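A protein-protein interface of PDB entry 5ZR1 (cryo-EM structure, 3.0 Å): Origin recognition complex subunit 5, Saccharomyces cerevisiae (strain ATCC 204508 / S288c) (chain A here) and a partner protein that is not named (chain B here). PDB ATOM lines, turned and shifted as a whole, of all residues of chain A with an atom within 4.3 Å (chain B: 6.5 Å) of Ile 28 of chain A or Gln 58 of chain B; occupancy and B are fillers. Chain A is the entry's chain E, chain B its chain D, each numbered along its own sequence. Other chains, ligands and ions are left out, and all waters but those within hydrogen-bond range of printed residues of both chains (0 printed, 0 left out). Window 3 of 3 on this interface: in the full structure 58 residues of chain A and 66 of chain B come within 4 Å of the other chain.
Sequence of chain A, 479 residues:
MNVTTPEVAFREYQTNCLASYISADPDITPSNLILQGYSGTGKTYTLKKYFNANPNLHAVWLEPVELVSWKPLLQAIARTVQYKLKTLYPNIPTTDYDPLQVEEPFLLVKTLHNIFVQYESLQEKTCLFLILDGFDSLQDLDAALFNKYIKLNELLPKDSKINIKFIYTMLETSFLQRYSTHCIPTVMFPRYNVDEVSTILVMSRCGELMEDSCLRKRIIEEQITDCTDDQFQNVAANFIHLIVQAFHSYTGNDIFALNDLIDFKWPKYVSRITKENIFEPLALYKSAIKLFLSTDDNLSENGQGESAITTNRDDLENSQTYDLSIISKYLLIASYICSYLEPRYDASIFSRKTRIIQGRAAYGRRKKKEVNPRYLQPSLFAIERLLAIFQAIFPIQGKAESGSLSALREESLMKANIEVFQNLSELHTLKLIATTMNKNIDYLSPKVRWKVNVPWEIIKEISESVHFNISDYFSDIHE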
ATOM      1  N   MET A   1       8.287 -22.409  -7.321  1.00  0.00           N
ATOM      2  CA  MET A   1       7.629 -21.148  -7.002  1.00  0.00           C
ATOM      3  C   MET A   1       8.580 -20.215  -6.266  1.00  0.00           C
ATOM      4  O   MET A   1       9.628 -19.834  -6.786  1.00  0.00           O
ATOM      5  CB  MET A   1       6.387 -21.389  -6.144  1.00  0.00           C
ATOM      6  CG  MET A   1       5.256 -22.132  -6.805  1.00  0.00           C
ATOM      7  SD  MET A   1       3.981 -22.325  -5.557  1.00  0.00           S
ATOM      8  CE  MET A   1       2.779 -23.316  -6.411  1.00  0.00           C
ATOM      9  N   TYR A  21       0.862 -27.321  -3.719  1.00  0.00           N
ATOM     10  CA  TYR A  21      -0.443 -26.736  -3.456  1.00  0.00           C
ATOM     11  C   TYR A  21      -0.389 -25.588  -2.465  1.00  0.00           C
ATOM     12  O   TYR A  21      -1.192 -24.657  -2.568  1.00  0.00           O
ATOM     13  CB  TYR A  21      -1.417 -27.800  -2.949  1.00  0.00           C
ATOM     14  CG  TYR A  21      -1.749 -28.850  -3.977  1.00  0.00           C
ATOM     15  CD1 TYR A  21      -2.485 -28.529  -5.102  1.00  0.00           C
ATOM     16  CD2 TYR A  21      -1.375 -30.171  -3.795  1.00  0.00           C
ATOM     17  CE1 TYR A  21      -2.798 -29.480  -6.042  1.00  0.00           C
ATOM     18  CE2 TYR A  21      -1.688 -31.133  -4.726  1.00  0.00           C
ATOM     19  CZ  TYR A  21      -2.402 -30.782  -5.846  1.00  0.00           C
ATOM     20  OH  TYR A  21      -2.726 -31.735  -6.778  1.00  0.00           O
ATOM     21  N   SER A  23       1.199 -22.311  -0.887  1.00  0.00           N
ATOM     22  CA  SER A  23       2.061 -21.205  -1.268  1.00  0.00           C
ATOM     23  C   SER A  23       1.567 -19.948  -0.578  1.00  0.00           C
ATOM     24  O   SER A  23       0.503 -19.936   0.037  1.00  0.00           O
ATOM     25  CB  SER A  23       2.082 -21.007  -2.779  1.00  0.00           C
ATOM     26  OG  SER A  23       0.809 -20.607  -3.247  1.00  0.00           O
ATOM     27  N   ASP A  25       1.076 -16.993  -2.274  1.00  0.00           N
ATOM     28  CA  ASP A  25       0.212 -16.275  -3.204  1.00  0.00           C
ATOM     29  C   ASP A  25      -1.173 -16.911  -3.198  1.00  0.00           C
ATOM     30  O   ASP A  25      -1.293 -18.101  -3.504  1.00  0.00           O
ATOM     31  CB  ASP A  25       0.817 -16.322  -4.604  1.00  0.00           C
ATOM     32  CG  ASP A  25       0.197 -15.317  -5.561  1.00  0.00           C
ATOM     33  OD1 ASP A  25      -0.715 -14.567  -5.163  1.00  0.00           O
ATOM     34  OD2 ASP A  25       0.634 -15.276  -6.730  1.00  0.00           O
ATOM     35  N   PRO A  26      -2.235 -16.170  -2.861  1.00  0.00           N
ATOM     36  CA  PRO A  26      -3.564 -16.790  -2.764  1.00  0.00           C
ATOM     37  C   PRO A  26      -4.217 -17.118  -4.097  1.00  0.00           C
ATOM     38  O   PRO A  26      -5.220 -17.843  -4.103  1.00  0.00           O
ATOM     39  CB  PRO A  26      -4.384 -15.731  -2.017  1.00  0.00           C
ATOM     40  CG  PRO A  26      -3.389 -14.875  -1.341  1.00  0.00           C
ATOM     41  CD  PRO A  26      -2.230 -14.823  -2.276  1.00  0.00           C
ATOM     42  N   ASP A  27      -3.705 -16.608  -5.217  1.00  0.00           N
ATOM     43  CA  ASP A  27      -4.316 -16.911  -6.505  1.00  0.00           C
ATOM     44  C   ASP A  27      -3.970 -18.311  -6.991  1.00  0.00           C
ATOM     45  O   ASP A  27      -4.722 -18.890  -7.780  1.00  0.00           O
ATOM     46  CB  ASP A  27      -3.883 -15.888  -7.555  1.00  0.00           C
ATOM     47  CG  ASP A  27      -4.482 -14.522  -7.320  1.00  0.00           C
ATOM     48  OD1 ASP A  27      -5.580 -14.446  -6.733  1.00  0.00           O
ATOM     49  OD2 ASP A  27      -3.860 -13.522  -7.733  1.00  0.00           O
ATOM     50  N   ILE A  28      -2.849 -18.867  -6.539  1.00  0.00           N
ATOM     51  CA  ILE A  28      -2.368 -20.144  -7.048  1.00  0.00           C
ATOM     52  C   ILE A  28      -2.385 -21.193  -5.945  1.00  0.00           C
ATOM     53  O   ILE A  28      -1.596 -22.144  -5.959  1.00  0.00           O
ATOM     54  CB  ILE A  28      -0.966 -19.986  -7.661  1.00  0.00           C
ATOM     55  CG1 ILE A  28       0.009 -19.404  -6.637  1.00  0.00           C
ATOM     56  CG2 ILE A  28      -1.022 -19.091  -8.871  1.00  0.00           C
ATOM     57  CD1 ILE A  28       1.436 -19.383  -7.106  1.00  0.00           C
ATOM     58  N   THR A  29      -3.304 -21.044  -4.999  1.00  0.00           N
ATOM     59  CA  THR A  29      -3.489 -21.990  -3.918  1.00  0.00           C
ATOM     60  C   THR A  29      -4.938 -22.456  -3.913  1.00  0.00           C
ATOM     61  O   THR A  29      -5.845 -21.621  -4.035  1.00  0.00           O
ATOM     62  CB  THR A  29      -3.130 -21.340  -2.566  1.00  0.00           C
ATOM     63  OG1 THR A  29      -1.772 -20.892  -2.598  1.00  0.00           O
ATOM     64  CG2 THR A  29      -3.283 -22.317  -1.421  1.00  0.00           C
ATOM     65  N   GLN B  53       5.670 -20.085 -15.068  1.00  0.00           N
ATOM     66  CA  GLN B  53       4.895 -20.972 -14.208  1.00  0.00           C
ATOM     67  C   GLN B  53       3.676 -20.270 -13.639  1.00  0.00           C
ATOM     68  O   GLN B  53       2.579 -20.835 -13.633  1.00  0.00           O
ATOM     69  CB  GLN B  53       5.735 -21.514 -13.056  1.00  0.00           C
ATOM     70  CG  GLN B  53       6.629 -22.673 -13.364  1.00  0.00           C
ATOM     71  CD  GLN B  53       7.246 -23.231 -12.099  1.00  0.00           C
ATOM     72  OE1 GLN B  53       7.104 -22.648 -11.028  1.00  0.00           O
ATOM     73  NE2 GLN B  53       7.888 -24.383 -12.207  1.00  0.00           N
ATOM     74  N   ARG B  54       3.852 -19.035 -13.157  1.00  0.00           N
ATOM     75  CA  ARG B  54       2.841 -18.405 -12.316  1.00  0.00           C
ATOM     76  C   ARG B  54       1.581 -18.050 -13.093  1.00  0.00           C
ATOM     77  O   ARG B  54       0.479 -18.177 -12.554  1.00  0.00           O
ATOM     78  CB  ARG B  54       3.427 -17.168 -11.637  1.00  0.00           C
ATOM     79  CG  ARG B  54       2.520 -16.538 -10.592  1.00  0.00           C
ATOM     80  CD  ARG B  54       3.195 -15.377  -9.889  1.00  0.00           C
ATOM     81  NE  ARG B  54       4.342 -15.811  -9.097  1.00  0.00           N
ATOM     82  CZ  ARG B  54       5.602 -15.486  -9.368  1.00  0.00           C
ATOM     83  NH1 ARG B  54       5.881 -14.721 -10.414  1.00  0.00           N
ATOM     84  NH2 ARG B  54       6.583 -15.926  -8.592  1.00  0.00           N
ATOM     85  N   ARG B  55       1.704 -17.646 -14.359  1.00  0.00           N
ATOM     86  CA  ARG B  55       0.494 -17.452 -15.151  1.00  0.00           C
ATOM     87  C   ARG B  55      -0.127 -18.782 -15.538  1.00  0.00           C
ATOM     88  O   ARG B  55      -1.343 -18.967 -15.406  1.00  0.00           O
ATOM     89  CB  ARG B  55       0.767 -16.639 -16.407  1.00  0.00           C
ATOM     90  CG  ARG B  55      -0.529 -16.384 -17.155  1.00  0.00           C
ATOM     91  CD  ARG B  55      -0.348 -15.583 -18.391  1.00  0.00           C
ATOM     92  NE  ARG B  55      -1.606 -15.396 -19.105  1.00  0.00           N
ATOM     93  CZ  ARG B  55      -2.451 -14.403 -18.865  1.00  0.00           C
ATOM     94  NH1 ARG B  55      -3.571 -14.300 -19.561  1.00  0.00           N
ATOM     95  NH2 ARG B  55      -2.168 -13.508 -17.930  1.00  0.00           N
ATOM     96  N   LEU B  56       0.699 -19.725 -15.993  1.00  0.00           N
ATOM     97  CA  LEU B  56       0.225 -21.022 -16.458  1.00  0.00           C
ATOM     98  C   LEU B  56      -0.398 -21.835 -15.339  1.00  0.00           C
ATOM     99  O   LEU B  56      -1.222 -22.713 -15.607  1.00  0.00           O
ATOM    100  CB  LEU B  56       1.394 -21.783 -17.065  1.00  0.00           C
ATOM    101  CG  LEU B  56       1.254 -22.912 -18.065  1.00  0.00           C
ATOM    102  CD1 LEU B  56       2.530 -22.870 -18.843  1.00  0.00           C
ATOM    103  CD2 LEU B  56       1.093 -24.252 -17.414  1.00  0.00           C
ATOM    104  N   LEU B  57      -0.030 -21.549 -14.098  1.00  0.00           N
ATOM    105  CA  LEU B  57      -0.662 -22.174 -12.955  1.00  0.00           C
ATOM    106  C   LEU B  57      -1.900 -21.420 -12.501  1.00  0.00           C
ATOM    107  O   LEU B  57      -2.844 -22.049 -12.021  1.00  0.00           O
ATOM    108  CB  LEU B  57       0.344 -22.281 -11.812  1.00  0.00           C
ATOM    109  CG  LEU B  57       0.025 -23.186 -10.642  1.00  0.00           C
ATOM    110  CD1 LEU B  57      -0.107 -24.593 -11.143  1.00  0.00           C
ATOM    111  CD2 LEU B  57       1.167 -23.096  -9.697  1.00  0.00           C
ATOM    112  N   GLN B  58      -1.946 -20.095 -12.658  1.00  0.00           N
ATOM    113  CA  GLN B  58      -3.161 -19.366 -12.319  1.00  0.00           C
ATOM    114  C   GLN B  58      -4.169 -19.343 -13.456  1.00  0.00           C
ATOM    115  O   GLN B  58      -5.286 -18.861 -13.259  1.00  0.00           O
ATOM    116  CB  GLN B  58      -2.854 -17.927 -11.885  1.00  0.00           C
ATOM    117  CG  GLN B  58      -2.497 -16.956 -12.982  1.00  0.00           C
ATOM    118  CD  GLN B  58      -2.066 -15.614 -12.427  1.00  0.00           C
ATOM    119  OE1 GLN B  58      -2.077 -15.403 -11.218  1.00  0.00           O
ATOM    120  NE2 GLN B  58      -1.672 -14.705 -13.308  1.00  0.00           N
ATOM    121  N   GLN B  59      -3.804 -19.835 -14.640  1.00  0.00           N
ATOM    122  CA  GLN B  59      -4.821 -20.209 -15.615  1.00  0.00           C
ATOM    123  C   GLN B  59      -5.495 -21.513 -15.225  1.00  0.00           C
ATOM    124  O   GLN B  59      -6.662 -21.731 -15.562  1.00  0.00           O
ATOM    125  CB  GLN B  59      -4.217 -20.340 -17.013  1.00  0.00           C
ATOM    126  CG  GLN B  59      -3.791 -19.032 -17.629  1.00  0.00           C
ATOM    127  CD  GLN B  59      -3.250 -19.197 -19.028  1.00  0.00           C
ATOM    128  OE1 GLN B  59      -3.080 -20.308 -19.512  1.00  0.00           O
ATOM    129  NE2 GLN B  59      -2.989 -18.083 -19.694  1.00  0.00           N
ATOM    130  N   LEU B  60      -4.771 -22.383 -14.525  1.00  0.00           N
ATOM    131  CA  LEU B  60      -5.296 -23.644 -14.029  1.00  0.00           C
ATOM    132  C   LEU B  60      -6.130 -23.493 -12.768  1.00  0.00           C
ATOM    133  O   LEU B  60      -6.758 -24.465 -12.348  1.00  0.00           O
ATOM    134  CB  LEU B  60      -4.149 -24.615 -13.767  1.00  0.00           C
ATOM    135  CG  LEU B  60      -3.465 -25.180 -15.005  1.00  0.00           C
ATOM    136  CD1 LEU B  60      -2.188 -25.886 -14.631  1.00  0.00           C
ATOM    137  CD2 LEU B  60      -4.409 -26.146 -15.678  1.00  0.00           C
ATOM    138  N   TYR B  61      -6.139 -22.324 -12.134  1.00  0.00           N
ATOM    139  CA  TYR B  61      -7.074 -22.059 -11.054  1.00  0.00           C
ATOM    140  C   TYR B  61      -8.184 -21.104 -11.453  1.00  0.00           C
ATOM    141  O   TYR B  61      -9.169 -20.987 -10.719  1.00  0.00           O
ATOM    142  CB  TYR B  61      -6.348 -21.502  -9.822  1.00  0.00           C
ATOM    143  CG  TYR B  61      -5.534 -22.530  -9.078  1.00  0.00           C
ATOM    144  CD1 TYR B  61      -6.134 -23.411  -8.195  1.00  0.00           C
ATOM    145  CD2 TYR B  61      -4.168 -22.616  -9.257  1.00  0.00           C
ATOM    146  CE1 TYR B  61      -5.392 -24.350  -7.516  1.00  0.00           C
ATOM    147  CE2 TYR B  61      -3.417 -23.550  -8.586  1.00  0.00           C
ATOM    148  CZ  TYR B  61      -4.035 -24.414  -7.719  1.00  0.00           C
ATOM    149  OH  TYR B  61      -3.287 -25.345  -7.045  1.00  0.00           O
ATOM    150  N   GLY B  62      -8.058 -20.432 -12.590  1.00  0.00           N
ATOM    151  CA  GLY B  62      -9.069 -19.498 -13.024  1.00  0.00           C
ATOM    152  C   GLY B  62      -8.997 -18.138 -12.377  1.00  0.00           C
ATOM    153  O   GLY B  62      -9.977 -17.391 -12.439  1.00  0.00           O
ATOM    154  N   THR B  63      -7.871 -17.790 -11.760  1.00  0.00           N
ATOM    155  CA  THR B  63      -7.712 -16.507 -11.095  1.00  0.00           C
ATOM    156  C   THR B  63      -7.098 -15.447 -12.000  1.00  0.00           C
ATOM    157  O   THR B  63      -6.440 -14.526 -11.506  1.00  0.00           O
ATOM    158  CB  THR B  63      -6.881 -16.673  -9.826  1.00  0.00           C
ATOM    159  OG1 THR B  63      -5.603 -17.220 -10.160  1.00  0.00           O
ATOM    160  CG2 THR B  63      -7.586 -17.601  -8.861  1.00  0.00           C
ATOM    161  N   LEU B  64      -7.294 -15.565 -13.309  1.00  0.00           N
ATOM    162  CA  LEU B  64      -7.004 -14.473 -14.217  1.00  0.00           C
ATOM    163  C   LEU B  64      -8.008 -13.342 -13.990  1.00  0.00           C
ATOM    164  O   LEU B  64      -9.119 -13.583 -13.514  1.00  0.00           O
ATOM    165  CB  LEU B  64      -7.083 -14.956 -15.661  1.00  0.00           C
ATOM    166  CG  LEU B  64      -6.054 -15.978 -16.124  1.00  0.00           C
ATOM    167  CD1 LEU B  64      -6.366 -16.382 -17.545  1.00  0.00           C
ATOM    168  CD2 LEU B  64      -4.651 -15.416 -16.011  1.00  0.00           C
ATOM    169  N   PRO B  65      -7.641 -12.097 -14.303  1.00  0.00           N
ATOM    170  CA  PRO B  65      -8.620 -11.008 -14.211  1.00  0.00           C
ATOM    171  C   PRO B  65      -9.699 -11.131 -15.274  1.00  0.00           C
ATOM    172  O   PRO B  65      -9.481 -11.676 -16.359  1.00  0.00           O
ATOM    173  CB  PRO B  65      -7.772  -9.749 -14.417  1.00  0.00           C
ATOM    174  CG  PRO B  65      -6.584 -10.213 -15.154  1.00  0.00           C
ATOM    175  CD  PRO B  65      -6.300 -11.587 -14.643  1.00  0.00           C
ATOM    176  N   ILE B 342      -1.578 -29.508 -12.384  1.00  0.00           N
ATOM    177  CA  ILE B 342      -1.073 -28.461 -11.482  1.00  0.00           C
ATOM    178  C   ILE B 342       0.248 -28.823 -10.799  1.00  0.00           C
ATOM    179  O   ILE B 342       1.166 -27.988 -10.817  1.00  0.00           O
ATOM    180  CB  ILE B 342      -2.182 -28.023 -10.506  1.00  0.00           C
ATOM    181  CG1 ILE B 342      -3.177 -27.091 -11.186  1.00  0.00           C
ATOM    182  CG2 ILE B 342      -1.618 -27.396  -9.241  1.00  0.00           C
ATOM    183  CD1 ILE B 342      -4.404 -26.836 -10.371  1.00  0.00           C
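N of Thr 63 of chain B lies within hydrogen-bond range of O of Gln 58 of chain B, 3.2 Å away.
Printed residues of chain B within 4 Å of Tyr 21 of chain A: Tyr 61 and Ile 342. Pro 26 of chain A touches none of the printed residues of chain B. Of the printed residues of chain B, Ile 28 of chain A touches Gln 58 (3.7 Å) and Tyr 61 (3.5 Å). Of the printed residues of chain A, Leu 57 of chain B touches Met 1 (3.7 Å). Gln 58 of chain B touches one residue of chain A. Pro 65 of chain B touches none of the printed residues of chain A. Printed residues of chain A within 4 Å of Ile 342 of chain B: Tyr 21 (3.996 Å). The nearest residue of chain B that does not touch Ile 28 of chain A is Arg 54 of chain B (4.1 Å).
O of Asp 27 of chain A sits at hydrogen-bond distance from OG1 of Thr 63 of chain B, at 3.0 Å.
Of the 14 printed residues of chain B, 6 touch a printed residue of chain A. Hydrophobic or aromatic side chains of chain B within 4 Å of the printed part of chain A: Leu 57, Tyr 61 and Ile 342. Of the 8 printed residues of chain A, 4 touch a printed residue of chain B. Among the printed residues, 8 pairs touch across the chains. Among the printed residues, no Asp or Glu carboxylate lies within 4 Å of a Lys or Arg side-chain nitrogen of the other chain.
Among the printed residues, pairs that only touch across the chains: Met 1 of chain A with Gln 53 of chain B (3.9 Å), Met 1 of chain A with Leu 57 of chain B (3.7 Å), Tyr 21 of chain A with Tyr 61 of chain B (3.8 Å), Tyr 21 of chain A with Ile 342 of chain B (3.996 Å), Asp 27 of chain A with Tyr 61 of chain B (3.7 Å), Ile 28 of chain A with Gln 58 of chain B (3.7 Å) and Ile 28 of chain A with Tyr 61 of chain B (3.5 Å).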
